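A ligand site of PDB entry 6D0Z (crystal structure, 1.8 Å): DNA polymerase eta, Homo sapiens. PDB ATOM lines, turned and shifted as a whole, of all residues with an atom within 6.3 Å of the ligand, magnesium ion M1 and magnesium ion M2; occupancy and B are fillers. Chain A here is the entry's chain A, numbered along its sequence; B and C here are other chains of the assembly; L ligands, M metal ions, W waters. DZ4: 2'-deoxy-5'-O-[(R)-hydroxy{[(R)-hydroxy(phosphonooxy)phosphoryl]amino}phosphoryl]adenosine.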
ATOM      1  N   VAL A  15       4.755  15.008 -16.980  1.00  0.00           N
ATOM      2  CA  VAL A  15       4.582  16.147 -17.881  1.00  0.00           C
ATOM      3  C   VAL A  15       5.853  16.272 -18.713  1.00  0.00           C
ATOM      4  O   VAL A  15       6.958  16.282 -18.179  1.00  0.00           O
ATOM      5  CB  VAL A  15       4.307  17.437 -17.083  1.00  0.00           C
ATOM      6  CG1 VAL A  15       4.172  18.630 -18.025  1.00  0.00           C
ATOM      7  CG2 VAL A  15       3.052  17.280 -16.242  1.00  0.00           C
ATOM      8  N   ASP A  16       5.683  16.372 -20.030  1.00  0.00           N
ATOM      9  CA  ASP A  16       6.793  16.430 -20.983  1.00  0.00           C
ATOM     10  C   ASP A  16       6.517  17.574 -21.948  1.00  0.00           C
ATOM     11  O   ASP A  16       5.553  17.510 -22.712  1.00  0.00           O
ATOM     12  CB  ASP A  16       6.921  15.094 -21.731  1.00  0.00           C
ATOM     13  CG  ASP A  16       8.145  15.033 -22.637  1.00  0.00           C
ATOM     14  OD1 ASP A  16       8.643  16.091 -23.067  1.00  0.00           O
ATOM     15  OD2 ASP A  16       8.585  13.900 -22.933  1.00  0.00           O
ATOM     16  N   MET A  17       7.349  18.614 -21.913  1.00  0.00           N
ATOM     17  CA  MET A  17       7.119  19.762 -22.779  1.00  0.00           C
ATOM     18  C   MET A  17       7.237  19.334 -24.236  1.00  0.00           C
ATOM     19  O   MET A  17       8.045  18.475 -24.591  1.00  0.00           O
ATOM     20  CB  MET A  17       8.121  20.887 -22.493  1.00  0.00           C
ATOM     21  CG  MET A  17       8.210  21.333 -21.041  1.00  0.00           C
ATOM     22  SD  MET A  17       6.623  21.823 -20.334  1.00  0.00           S
ATOM     23  CE  MET A  17       6.219  23.281 -21.278  1.00  0.00           C
ATOM     24  N   ASP A  18       6.403  19.932 -25.091  1.00  0.00           N
ATOM     25  CA  ASP A  18       6.437  19.657 -26.514  1.00  0.00           C
ATOM     26  C   ASP A  18       7.567  20.444 -27.178  1.00  0.00           C
ATOM     27  O   ASP A  18       7.776  21.617 -26.867  1.00  0.00           O
ATOM     28  CB  ASP A  18       5.104  20.012 -27.179  1.00  0.00           C
ATOM     29  CG  ASP A  18       3.932  19.192 -26.637  1.00  0.00           C
ATOM     30  OD1 ASP A  18       4.138  18.031 -26.217  1.00  0.00           O
ATOM     31  OD2 ASP A  18       2.800  19.704 -26.657  1.00  0.00           O
ATOM     32  N   CYS A  19       8.281  19.788 -28.101  1.00  0.00           N
ATOM     33  CA  CYS A  19       9.440  20.339 -28.790  1.00  0.00           C
ATOM     34  C   CYS A  19      10.048  21.514 -28.016  1.00  0.00           C
ATOM     35  O   CYS A  19      10.020  22.658 -28.470  1.00  0.00           O
ATOM     36  CB  CYS A  19       9.075  20.759 -30.227  1.00  0.00           C
ATOM     37  SG  CYS A  19       7.652  21.873 -30.434  1.00  0.00           S
ATOM     38  N   PHE A  20      10.634  21.216 -26.849  1.00  0.00           N
ATOM     39  CA  PHE A  20      10.831  22.239 -25.828  1.00  0.00           C
ATOM     40  C   PHE A  20      11.728  23.388 -26.306  1.00  0.00           C
ATOM     41  O   PHE A  20      11.333  24.551 -26.256  1.00  0.00           O
ATOM     42  CB  PHE A  20      11.407  21.623 -24.562  1.00  0.00           C
ATOM     43  CG  PHE A  20      11.572  22.599 -23.439  1.00  0.00           C
ATOM     44  CD1 PHE A  20      10.526  23.435 -23.074  1.00  0.00           C
ATOM     45  CD2 PHE A  20      12.761  22.692 -22.739  1.00  0.00           C
ATOM     46  CE1 PHE A  20      10.662  24.334 -22.040  1.00  0.00           C
ATOM     47  CE2 PHE A  20      12.908  23.592 -21.696  1.00  0.00           C
ATOM     48  CZ  PHE A  20      11.859  24.413 -21.346  1.00  0.00           C
ATOM     49  N   PHE A  21      12.955  23.080 -26.727  1.00  0.00           N
ATOM     50  CA  PHE A  21      13.856  24.167 -27.102  1.00  0.00           C
ATOM     51  C   PHE A  21      13.279  24.980 -28.250  1.00  0.00           C
ATOM     52  O   PHE A  21      13.534  26.186 -28.343  1.00  0.00           O
ATOM     53  CB  PHE A  21      15.244  23.670 -27.503  1.00  0.00           C
ATOM     54  CG  PHE A  21      16.080  23.123 -26.358  1.00  0.00           C
ATOM     55  CD1 PHE A  21      15.535  22.796 -25.139  1.00  0.00           C
ATOM     56  CD2 PHE A  21      17.442  22.946 -26.539  1.00  0.00           C
ATOM     57  CE1 PHE A  21      16.331  22.289 -24.119  1.00  0.00           C
ATOM     58  CE2 PHE A  21      18.239  22.446 -25.532  1.00  0.00           C
ATOM     59  CZ  PHE A  21      17.684  22.120 -24.312  1.00  0.00           C
ATOM     60  N   VAL A  22      12.506  24.348 -29.132  1.00  0.00           N
ATOM     61  CA  VAL A  22      11.845  25.069 -30.211  1.00  0.00           C
ATOM     62  C   VAL A  22      10.849  26.077 -29.651  1.00  0.00           C
ATOM     63  O   VAL A  22      10.783  27.230 -30.094  1.00  0.00           O
ATOM     64  CB  VAL A  22      11.161  24.096 -31.186  1.00  0.00           C
ATOM     65  CG1 VAL A  22      10.194  24.827 -32.121  1.00  0.00           C
ATOM     66  CG2 VAL A  22      12.200  23.356 -32.012  1.00  0.00           C
ATOM     67  N   GLN A  41      22.928  23.430 -32.743  1.00  0.00           N
ATOM     68  CA  GLN A  41      24.116  23.938 -32.076  1.00  0.00           C
ATOM     69  C   GLN A  41      25.318  23.871 -33.010  1.00  0.00           C
ATOM     70  O   GLN A  41      25.538  22.878 -33.705  1.00  0.00           O
ATOM     71  CB  GLN A  41      24.421  23.205 -30.746  1.00  0.00           C
ATOM     72  CG  GLN A  41      24.225  21.704 -30.684  1.00  0.00           C
ATOM     73  CD  GLN A  41      24.349  21.185 -29.244  1.00  0.00           C
ATOM     74  OE1 GLN A  41      24.193  21.945 -28.285  1.00  0.00           O
ATOM     75  NE2 GLN A  41      24.642  19.909 -29.102  1.00  0.00           N
ATOM     76  N   ILE A  51      19.054  19.605 -32.521  1.00  0.00           N
ATOM     77  CA  ILE A  51      18.704  18.977 -31.251  1.00  0.00           C
ATOM     78  C   ILE A  51      17.219  19.058 -30.933  1.00  0.00           C
ATOM     79  O   ILE A  51      16.762  18.328 -30.030  1.00  0.00           O
ATOM     80  CB  ILE A  51      19.534  19.557 -30.075  1.00  0.00           C
ATOM     81  CG1 ILE A  51      19.377  21.079 -29.949  1.00  0.00           C
ATOM     82  CG2 ILE A  51      21.004  19.181 -30.258  1.00  0.00           C
ATOM     83  CD1 ILE A  51      20.013  21.627 -28.670  1.00  0.00           C
ATOM     84  N   ALA A  52      16.431  19.868 -31.638  1.00  0.00           N
ATOM     85  CA  ALA A  52      14.992  19.945 -31.408  1.00  0.00           C
ATOM     86  C   ALA A  52      14.293  20.384 -32.690  1.00  0.00           C
ATOM     87  O   ALA A  52      14.845  21.157 -33.480  1.00  0.00           O
ATOM     88  CB  ALA A  52      14.660  20.921 -30.265  1.00  0.00           C
ATOM     89  N   VAL A  53      13.069  19.886 -32.884  1.00  0.00           N
ATOM     90  CA  VAL A  53      12.363  19.995 -34.169  1.00  0.00           C
ATOM     91  C   VAL A  53      10.891  20.277 -33.915  1.00  0.00           C
ATOM     92  O   VAL A  53      10.220  19.538 -33.176  1.00  0.00           O
ATOM     93  CB  VAL A  53      12.538  18.719 -35.003  1.00  0.00           C
ATOM     94  CG1 VAL A  53      11.918  18.888 -36.390  1.00  0.00           C
ATOM     95  CG2 VAL A  53      13.999  18.328 -35.108  1.00  0.00           C
ATOM     96  N   TYR A  55       6.867  20.413 -34.792  1.00  0.00           N
ATOM     97  CA  TYR A  55       6.046  19.365 -35.373  1.00  0.00           C
ATOM     98  C   TYR A  55       5.764  19.624 -36.843  1.00  0.00           C
ATOM     99  O   TYR A  55       5.623  18.681 -37.621  1.00  0.00           O
ATOM    100  CB  TYR A  55       4.761  19.216 -34.553  1.00  0.00           C
ATOM    101  CG  TYR A  55       5.015  18.391 -33.305  1.00  0.00           C
ATOM    102  CD1 TYR A  55       5.559  18.973 -32.163  1.00  0.00           C
ATOM    103  CD2 TYR A  55       4.768  17.021 -33.289  1.00  0.00           C
ATOM    104  CE1 TYR A  55       5.821  18.224 -31.035  1.00  0.00           C
ATOM    105  CE2 TYR A  55       5.029  16.263 -32.157  1.00  0.00           C
ATOM    106  CZ  TYR A  55       5.554  16.861 -31.039  1.00  0.00           C
ATOM    107  OH  TYR A  55       5.815  16.110 -29.920  1.00  0.00           O
ATOM    108  N   ARG A  58       8.838  18.112 -38.409  1.00  0.00           N
ATOM    109  CA  ARG A  58       8.841  16.644 -38.346  1.00  0.00           C
ATOM    110  C   ARG A  58       8.047  16.028 -39.483  1.00  0.00           C
ATOM    111  O   ARG A  58       8.371  14.917 -39.932  1.00  0.00           O
ATOM    112  CB  ARG A  58       8.278  16.177 -37.009  1.00  0.00           C
ATOM    113  CG  ARG A  58       9.061  16.663 -35.820  1.00  0.00           C
ATOM    114  CD  ARG A  58       8.525  16.128 -34.516  1.00  0.00           C
ATOM    115  NE  ARG A  58       9.078  16.882 -33.397  1.00  0.00           N
ATOM    116  CZ  ARG A  58       9.046  16.510 -32.133  1.00  0.00           C
ATOM    117  NH1 ARG A  58       8.480  15.372 -31.787  1.00  0.00           N
ATOM    118  NH2 ARG A  58       9.601  17.276 -31.207  1.00  0.00           N
ATOM    119  N   ARG A  64      16.009  15.088 -34.685  1.00  0.00           N
ATOM    120  CA  ARG A  64      17.184  15.300 -33.852  1.00  0.00           C
ATOM    121  C   ARG A  64      18.358  14.482 -34.363  1.00  0.00           C
ATOM    122  O   ARG A  64      18.193  13.394 -34.915  1.00  0.00           O
ATOM    123  CB  ARG A  64      16.855  14.917 -32.407  1.00  0.00           C
ATOM    124  CG  ARG A  64      18.024  14.876 -31.442  1.00  0.00           C
ATOM    125  CD  ARG A  64      17.539  14.441 -30.070  1.00  0.00           C
ATOM    126  NE  ARG A  64      16.977  13.095 -30.134  1.00  0.00           N
ATOM    127  CZ  ARG A  64      15.904  12.686 -29.455  1.00  0.00           C
ATOM    128  NH1 ARG A  64      15.243  13.514 -28.664  1.00  0.00           N
ATOM    129  NH2 ARG A  64      15.478  11.443 -29.596  1.00  0.00           N
ATOM    130  N   SER A 116      14.166  15.520 -16.280  1.00  0.00           N
ATOM    131  CA  SER A 116      15.054  16.020 -17.325  1.00  0.00           C
ATOM    132  C   SER A 116      14.852  17.519 -17.419  1.00  0.00           C
ATOM    133  O   SER A 116      14.098  18.104 -16.638  1.00  0.00           O
ATOM    134  CB  SER A 116      14.780  15.351 -18.668  1.00  0.00           C
ATOM    135  OG  SER A 116      13.606  15.899 -19.252  1.00  0.00           O
ATOM    136  N   ILE A 117      15.492  18.151 -18.405  1.00  0.00           N
ATOM    137  CA  ILE A 117      15.349  19.594 -18.551  1.00  0.00           C
ATOM    138  C   ILE A 117      13.899  19.987 -18.827  1.00  0.00           C
ATOM    139  O   ILE A 117      13.511  21.117 -18.515  1.00  0.00           O
ATOM    140  CB  ILE A 117      16.293  20.135 -19.635  1.00  0.00           C
ATOM    141  CG1 ILE A 117      16.370  21.658 -19.523  1.00  0.00           C
ATOM    142  CG2 ILE A 117      15.837  19.723 -21.028  1.00  0.00           C
ATOM    143  CD1 ILE A 117      17.526  22.275 -20.274  1.00  0.00           C
ATOM    144  N   ASP A 118      13.085  19.089 -19.402  1.00  0.00           N
ATOM    145  CA  ASP A 118      11.730  19.474 -19.791  1.00  0.00           C
ATOM    146  C   ASP A 118      10.662  18.470 -19.372  1.00  0.00           C
ATOM    147  O   ASP A 118       9.559  18.482 -19.934  1.00  0.00           O
ATOM    148  CB  ASP A 118      11.633  19.701 -21.302  1.00  0.00           C
ATOM    149  CG  ASP A 118      11.373  18.419 -22.068  1.00  0.00           C
ATOM    150  OD1 ASP A 118      11.843  17.366 -21.614  1.00  0.00           O
ATOM    151  OD2 ASP A 118      10.698  18.462 -23.116  1.00  0.00           O
ATOM    152  N   GLU A 119      10.924  17.595 -18.404  1.00  0.00           N
ATOM    153  CA  GLU A 119       9.833  16.777 -17.881  1.00  0.00           C
ATOM    154  C   GLU A 119      10.000  16.545 -16.386  1.00  0.00           C
ATOM    155  O   GLU A 119      11.100  16.581 -15.838  1.00  0.00           O
ATOM    156  CB  GLU A 119       9.706  15.434 -18.611  1.00  0.00           C
ATOM    157  CG  GLU A 119      10.907  14.544 -18.545  1.00  0.00           C
ATOM    158  CD  GLU A 119      10.980  13.614 -19.738  1.00  0.00           C
ATOM    159  OE1 GLU A 119      10.154  12.687 -19.851  1.00  0.00           O
ATOM    160  OE2 GLU A 119      11.850  13.835 -20.601  1.00  0.00           O
ATOM    161  N   LYS A 227       4.768   7.773 -18.044  1.00  0.00           N
ATOM    162  CA  LYS A 227       5.662   8.147 -19.146  1.00  0.00           C
ATOM    163  C   LYS A 227       5.187   7.542 -20.456  1.00  0.00           C
ATOM    164  O   LYS A 227       5.161   8.220 -21.492  1.00  0.00           O
ATOM    165  CB  LYS A 227       7.084   7.700 -18.818  1.00  0.00           C
ATOM    166  CG  LYS A 227       8.087   7.831 -19.961  1.00  0.00           C
ATOM    167  CD  LYS A 227       8.341   9.281 -20.318  1.00  0.00           C
ATOM    168  CE  LYS A 227       9.417   9.404 -21.382  1.00  0.00           C
ATOM    169  NZ  LYS A 227       9.669  10.834 -21.701  1.00  0.00           N
ATOM    170  N   LYS A 234       0.947  12.849 -27.751  1.00  0.00           N
ATOM    171  CA  LYS A 234       1.759  14.033 -28.031  1.00  0.00           C
ATOM    172  C   LYS A 234       1.511  14.536 -29.453  1.00  0.00           C
ATOM    173  O   LYS A 234       1.415  13.722 -30.371  1.00  0.00           O
ATOM    174  CB  LYS A 234       3.253  13.701 -27.873  1.00  0.00           C
ATOM    175  CG  LYS A 234       3.901  14.267 -26.631  1.00  0.00           C
ATOM    176  CD  LYS A 234       5.412  14.220 -26.731  1.00  0.00           C
ATOM    177  CE  LYS A 234       6.048  14.766 -25.461  1.00  0.00           C
ATOM    178  NZ  LYS A 234       5.983  16.256 -25.419  1.00  0.00           N
ATOM    179  N   PRO A 235       1.447  15.869 -29.668  1.00  0.00           N
ATOM    180  CA  PRO A 235       1.605  16.979 -28.723  1.00  0.00           C
ATOM    181  C   PRO A 235       0.307  17.607 -28.204  1.00  0.00           C
ATOM    182  O   PRO A 235      -0.775  17.387 -28.750  1.00  0.00           O
ATOM    183  CB  PRO A 235       2.352  18.015 -29.560  1.00  0.00           C
ATOM    184  CG  PRO A 235       1.775  17.832 -30.927  1.00  0.00           C
ATOM    185  CD  PRO A 235       1.490  16.346 -31.060  1.00  0.00           C
ATOM    186  P    DT B   3      29.152  11.683 -36.813  1.00  0.00           P
ATOM    187  OP1  DT B   3      29.898  10.502 -37.304  1.00  0.00           O
ATOM    188  OP2  DT B   3      27.874  12.057 -37.458  1.00  0.00           O
ATOM    189  O5'  DT B   3      28.893  11.498 -35.246  1.00  0.00           O
ATOM    190  C5'  DT B   3      27.696  11.985 -34.652  1.00  0.00           C
ATOM    191  C4'  DT B   3      27.827  13.454 -34.288  1.00  0.00           C
ATOM    192  O4'  DT B   3      26.501  13.999 -34.035  1.00  0.00           O
ATOM    193  C3'  DT B   3      28.640  13.741 -33.041  1.00  0.00           C
ATOM    194  O3'  DT B   3      29.354  14.973 -33.189  1.00  0.00           O
ATOM    195  C2'  DT B   3      27.577  13.804 -31.952  1.00  0.00           C
ATOM    196  C1'  DT B   3      26.411  14.439 -32.689  1.00  0.00           C
ATOM    197  N1   DT B   3      25.052  14.069 -32.161  1.00  0.00           N
ATOM    198  C2   DT B   3      24.209  15.068 -31.751  1.00  0.00           C
ATOM    199  O2   DT B   3      24.505  16.250 -31.767  1.00  0.00           O
ATOM    200  N3   DT B   3      22.979  14.641 -31.304  1.00  0.00           N
ATOM    201  C4   DT B   3      22.533  13.341 -31.236  1.00  0.00           C
ATOM    202  O4   DT B   3      21.418  13.058 -30.812  1.00  0.00           O
ATOM    203  C5   DT B   3      23.465  12.337 -31.685  1.00  0.00           C
ATOM    204  C7   DT B   3      23.083  10.888 -31.651  1.00  0.00           C
ATOM    205  C6   DT B   3      24.672  12.745 -32.135  1.00  0.00           C
ATOM    206  P    DT B   4      30.328  15.499 -32.011  1.00  0.00           P
ATOM    207  OP1  DT B   4      31.332  16.419 -32.588  1.00  0.00           O
ATOM    208  OP2  DT B   4      30.738  14.305 -31.234  1.00  0.00           O
ATOM    209  O5'  DT B   4      29.366  16.372 -31.098  1.00  0.00           O
ATOM    210  C5'  DT B   4      28.748  17.532 -31.622  1.00  0.00           C
ATOM    211  C4'  DT B   4      28.119  18.331 -30.510  1.00  0.00           C
ATOM    212  O4'  DT B   4      26.827  17.753 -30.167  1.00  0.00           O
ATOM    213  C3'  DT B   4      28.936  18.335 -29.219  1.00  0.00           C
ATOM    214  O3'  DT B   4      28.944  19.634 -28.684  1.00  0.00           O
ATOM    215  C2'  DT B   4      28.215  17.320 -28.337  1.00  0.00           C
ATOM    216  C1'  DT B   4      26.773  17.512 -28.773  1.00  0.00           C
ATOM    217  N1   DT B   4      25.852  16.350 -28.541  1.00  0.00           N
ATOM    218  C2   DT B   4      24.567  16.618 -28.144  1.00  0.00           C
ATOM    219  O2   DT B   4      24.153  17.749 -27.934  1.00  0.00           O
ATOM    220  N3   DT B   4      23.776  15.524 -27.967  1.00  0.00           N
ATOM    221  C4   DT B   4      24.127  14.203 -28.164  1.00  0.00           C
ATOM    222  O4   DT B   4      23.345  13.278 -27.988  1.00  0.00           O
ATOM    223  C5   DT B   4      25.488  13.975 -28.602  1.00  0.00           C
ATOM    224  C7   DT B   4      25.964  12.575 -28.852  1.00  0.00           C
ATOM    225  C6   DT B   4      26.276  15.056 -28.786  1.00  0.00           C
ATOM    226  P    DG B   5      29.749  19.963 -27.344  1.00  0.00           P
ATOM    227  OP1  DG B   5      30.230  21.357 -27.434  1.00  0.00           O
ATOM    228  OP2  DG B   5      30.669  18.853 -27.044  1.00  0.00           O
ATOM    229  O5'  DG B   5      28.599  19.929 -26.236  1.00  0.00           O
ATOM    230  C5'  DG B   5      27.496  20.809 -26.352  1.00  0.00           C
ATOM    231  C4'  DG B   5      26.553  20.607 -25.204  1.00  0.00           C
ATOM    232  O4'  DG B   5      25.819  19.356 -25.384  1.00  0.00           O
ATOM    233  C3'  DG B   5      27.232  20.495 -23.841  1.00  0.00           C
ATOM    234  O3'  DG B   5      26.461  21.157 -22.861  1.00  0.00           O
ATOM    235  C2'  DG B   5      27.276  18.986 -23.622  1.00  0.00           C
ATOM    236  C1'  DG B   5      25.923  18.612 -24.188  1.00  0.00           C
ATOM    237  N9   DG B   5      25.724  17.192 -24.466  1.00  0.00           N
ATOM    238  C8   DG B   5      26.649  16.259 -24.863  1.00  0.00           C
ATOM    239  N7   DG B   5      26.139  15.069 -25.043  1.00  0.00           N
ATOM    240  C5   DG B   5      24.790  15.230 -24.743  1.00  0.00           C
ATOM    241  C6   DG B   5      23.712  14.291 -24.752  1.00  0.00           C
ATOM    242  O6   DG B   5      23.754  13.089 -25.028  1.00  0.00           O
ATOM    243  N1   DG B   5      22.512  14.884 -24.390  1.00  0.00           N
ATOM    244  C2   DG B   5      22.352  16.208 -24.056  1.00  0.00           C
ATOM    245  N2   DG B   5      21.115  16.596 -23.722  1.00  0.00           N
ATOM    246  N3   DG B   5      23.339  17.089 -24.040  1.00  0.00           N
ATOM    247  C4   DG B   5      24.525  16.530 -24.401  1.00  0.00           C
ATOM    248  P   CAR C   8      13.291   9.799 -21.073  1.00  0.00           P
ATOM    249  OP1 CAR C   8      12.150  10.163 -20.142  1.00  0.00           O
ATOM    250  OP2 CAR C   8      13.015   9.314 -22.472  1.00  0.00           O
ATOM    251  O5' CAR C   8      14.219  11.079 -21.164  1.00  0.00           O
ATOM    252  C5' CAR C   8      13.913  12.141 -22.037  1.00  0.00           C
ATOM    253  C4' CAR C   8      14.638  13.394 -21.625  1.00  0.00           C
ATOM    254  O4' CAR C   8      16.066  13.103 -21.536  1.00  0.00           O
ATOM    255  C3' CAR C   8      14.497  14.556 -22.600  1.00  0.00           C
ATOM    256  O3' CAR C   8      14.502  15.786 -21.885  1.00  0.00           O
ATOM    257  C2' CAR C   8      15.765  14.435 -23.440  1.00  0.00           C
ATOM    258  O2' CAR C   8      15.682  13.499 -24.499  1.00  0.00           O
ATOM    259  C1' CAR C   8      16.773  13.975 -22.403  1.00  0.00           C
ATOM    260  N1  CAR C   8      17.886  13.246 -23.030  1.00  0.00           N
ATOM    261  C2  CAR C   8      19.040  13.964 -23.370  1.00  0.00           C
ATOM    262  O2  CAR C   8      19.103  15.183 -23.089  1.00  0.00           O
ATOM    263  N3  CAR C   8      20.073  13.352 -23.972  1.00  0.00           N
ATOM    264  C4  CAR C   8      19.992  12.034 -24.272  1.00  0.00           C
ATOM    265  N4  CAR C   8      21.023  11.418 -24.883  1.00  0.00           N
ATOM    266  C5  CAR C   8      18.856  11.313 -23.964  1.00  0.00           C
ATOM    267  C6  CAR C   8      17.787  11.948 -23.345  1.00  0.00           C
HETATM  268  N1  DZ4 L   1      21.247  16.209 -27.276  1.00  0.00           N
HETATM  269  C2  DZ4 L   1      21.082  17.509 -26.954  1.00  0.00           C
HETATM  270  N3  DZ4 L   1      19.889  18.027 -26.591  1.00  0.00           N
HETATM  271  C4  DZ4 L   1      18.790  17.241 -26.530  1.00  0.00           C
HETATM  272  C5  DZ4 L   1      18.893  15.821 -26.860  1.00  0.00           C
HETATM  273  C6  DZ4 L   1      20.222  15.328 -27.245  1.00  0.00           C
HETATM  274  N6  DZ4 L   1      20.354  14.015 -27.559  1.00  0.00           N
HETATM  275  N7  DZ4 L   1      17.669  15.282 -26.725  1.00  0.00           N
HETATM  276  C8  DZ4 L   1      16.837  16.292 -26.341  1.00  0.00           C
HETATM  277  N9  DZ4 L   1      17.511  17.454 -26.232  1.00  0.00           N
HETATM  278  PA  DZ4 L   1      12.794  15.812 -25.650  1.00  0.00           P
HETATM  279  PB  DZ4 L   1      11.287  17.655 -27.449  1.00  0.00           P
HETATM  280  PG  DZ4 L   1       8.836  16.231 -27.820  1.00  0.00           P
HETATM  281  C1' DZ4 L   1      16.967  18.770 -25.814  1.00  0.00           C
HETATM  282  O1A DZ4 L   1      11.597  15.812 -24.790  1.00  0.00           O
HETATM  283  O1B DZ4 L   1      10.805  18.196 -26.147  1.00  0.00           O
HETATM  284  O1G DZ4 L   1       8.995  16.128 -26.322  1.00  0.00           O
HETATM  285  C2' DZ4 L   1      16.182  19.430 -26.945  1.00  0.00           C
HETATM  286  O2A DZ4 L   1      13.274  14.346 -26.005  1.00  0.00           O
HETATM  287  O2B DZ4 L   1      12.060  18.782 -28.286  1.00  0.00           O
HETATM  288  O2G DZ4 L   1       7.668  17.065 -28.271  1.00  0.00           O
HETATM  289  C3' DZ4 L   1      14.741  19.112 -26.625  1.00  0.00           C
HETATM  290  O3' DZ4 L   1      13.823  20.112 -27.101  1.00  0.00           O
HETATM  291  N3A DZ4 L   1      12.428  16.385 -27.239  1.00  0.00           N
HETATM  292  O3B DZ4 L   1      10.094  17.077 -28.368  1.00  0.00           O
HETATM  293  O3G DZ4 L   1       9.010  14.922 -28.559  1.00  0.00           O
HETATM  294  C4' DZ4 L   1      14.747  19.000 -25.098  1.00  0.00           C
HETATM  295  O4' DZ4 L   1      16.058  18.550 -24.737  1.00  0.00           O
HETATM  296  C5' DZ4 L   1      13.701  18.037 -24.578  1.00  0.00           C
HETATM  297  O5' DZ4 L   1      13.977  16.710 -25.028  1.00  0.00           O
HETATM  298 MG    MG M   1       9.807  17.080 -24.564  1.00  0.00          MG
HETATM  299 MG    MG M   2      11.328  15.005 -22.295  1.00  0.00          MG
HETATM  300  O   HOH W   1      17.228  12.597 -26.432  1.00  0.00           O
HETATM  301  O   HOH W   2      14.824  16.473 -29.217  1.00  0.00           O
HETATM  302  O   HOH W   3      11.017  13.360 -23.617  1.00  0.00           O
HETATM  303  O   HOH W   4      17.882  17.613 -22.808  1.00  0.00           O
HETATM  304  O   HOH W   5      12.638  12.570 -27.694  1.00  0.00           O
HETATM  305  O   HOH W   6       6.673  13.131 -30.069  1.00  0.00           O
HETATM  306  O   HOH W   7      20.623  20.099 -24.792  1.00  0.00           O
HETATM  307  O   HOH W   8      12.277  17.978 -31.121  1.00  0.00           O
HETATM  308  O   HOH W   9       9.146  12.860 -26.592  1.00  0.00           O
HETATM  309  O   HOH W  10      11.252  13.924 -29.630  1.00  0.00           O
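O2A of the ligand lies within salt-bridge range of NH1 of Arg 64, at 3.4 Å.
O2G of the ligand is in salt-bridge range of NZ of Lys 234 (3.4 Å).
O2G of the ligand sits at hydrogen-bond distance from N of Cys 19.
N of Phe 20 sits at hydrogen-bond distance from O2B of the ligand (3.2 Å).
O2' of CAR 8 of chain C lies close to an oxygen (O2A) of the ligand, 3.0 Å away.
NH1 of Arg 58 is in salt-bridge range of O3G of the ligand (3.3 Å).
An oxygen (O3') of the ligand is in hydrogen-bond range of the backbone NH of Phe 21, 3.1 Å away.
The side-chain hydroxyl of Tyr 55 is in hydrogen-bond range of an oxygen (O2G) of the ligand, 2.7 Å away.
O4 of DT 4 of chain B lies within hydrogen-bond range of N6 of the ligand (3.1 Å).
OH of Tyr 55 lies within hydrogen-bond range of NH1 of Arg 58 (3.3 Å).
NZ of Lys 234 lies within hydrogen-bond range of O of Asp 16, 3.0 Å away.
OD2 of Asp 16 is in salt-bridge range of NZ of Lys 227, at 3.5 Å.
The side-chain amino group (NZ) of Lys 234 is in salt-bridge range of the side-chain carboxylate (OD1) of Asp 18 (2.7 Å).
OP1 of CAR 8 of chain C is in salt-bridge range of the side-chain amino group (NZ) of Lys 227, at 3.0 Å.
O2 of CAR 8 of chain C lies close to N2 of DG 5 of chain B, 2.5 Å away.
The side-chain amide nitrogen of Gln 41 is in hydrogen-bond range of O2 of DT 4 of chain B, 2.5 Å away.
The side-chain carboxylate of Glu 119 lies within salt-bridge range of the side-chain amino group of Lys 227, 2.7 Å away.
N1 of DG 5 of chain B sits close to N1 of the ligand (3.4 Å).
Residues that only touch the ligand: Asp 18 (3.4 Å), Ile 51 (3.3 Å), Ala 52 (3.4 Å), Ile 117 (3.9 Å) and DT 3 of chain B (3.6 Å).
Hydrophobic or aromatic side chains within 4 Å of the ligand: Phe 20, Phe 21, Ile 51, Ala 52, Tyr 55 and Ile 117.
18 residues have an atom within 4 Å of the ligand: Asp 16, Met 17, Asp 18, Cys 19, Phe 20, Phe 21, Ile 51, Ala 52, Tyr 55, Arg 58, Arg 64, Ile 117, Asp 118, Lys 234, DT 3 of chain B, DT 4 of chain B, DG 5 of chain B and CAR 8 of chain C.
The nearest printed residue that does not touch the ligand is Glu 119 (4.6 Å).
Three residues have an atom within 4 Å of magnesium ion M1: Asp 16, Met 17 and Asp 118.
Along chain A the residues within 4 Å of magnesium ion M1 span positions 16 to 118.
Ser 116 touches magnesium ion M2.
C3' of CAR 8 of chain C touches magnesium ion M2 (3.2 Å).
Magnesium ion M1 is bound by the side-chain carboxylate of Asp 16, an oxygen (O1G) of the ligand, an oxygen (O1B) of the ligand, the side-chain carboxylate of Asp 118, an oxygen (O1A) of the ligand and the backbone carbonyl oxygen of Met 17.
Magnesium ion M1 has six donor atoms within binding distance.
Magnesium ion M2 is bound by the side-chain carboxylate of Glu 119 (2.1 Å), water W3 (2.1 Å) and the side-chain carboxylate of Asp 118 (2.5 Å).
Slightly farther from magnesium ion M2 lies O1A of the ligand (2.6 Å).
Water W3 lies within hydrogen-bond range of OD2 of Asp 16 (2.6 Å), O2A of the ligand (3.4 Å) and NZ of Lys 227 (3.4 Å).
Water W5 bridges an oxygen (O2A) of the ligand (2.5 Å) and the guanidinium group (NH1) of Arg 64 (2.9 Å).
Water W1 lies within hydrogen-bond range of O2' of CAR 8 of chain C (2.6 Å), a nitrogen (N7) of the ligand (2.7 Å) and the guanidinium group (NH1) of Arg 64 (3.1 Å).
Water W4 lies within hydrogen-bond range of O2 of CAR 8 of chain C (2.7 Å) and an oxygen (O4') of the ligand (2.8 Å).
Water W8 lies within hydrogen-bond range of the backbone NH of Val 53 (2.7 Å), the guanidinium group of Arg 58 (2.8 Å) and an oxygen (O2B) of the ligand (3.0 Å).
Water W6 lies within hydrogen-bond range of the side-chain hydroxyl of Tyr 55, an oxygen (O3G) of the ligand and the guanidinium group of Arg 58.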
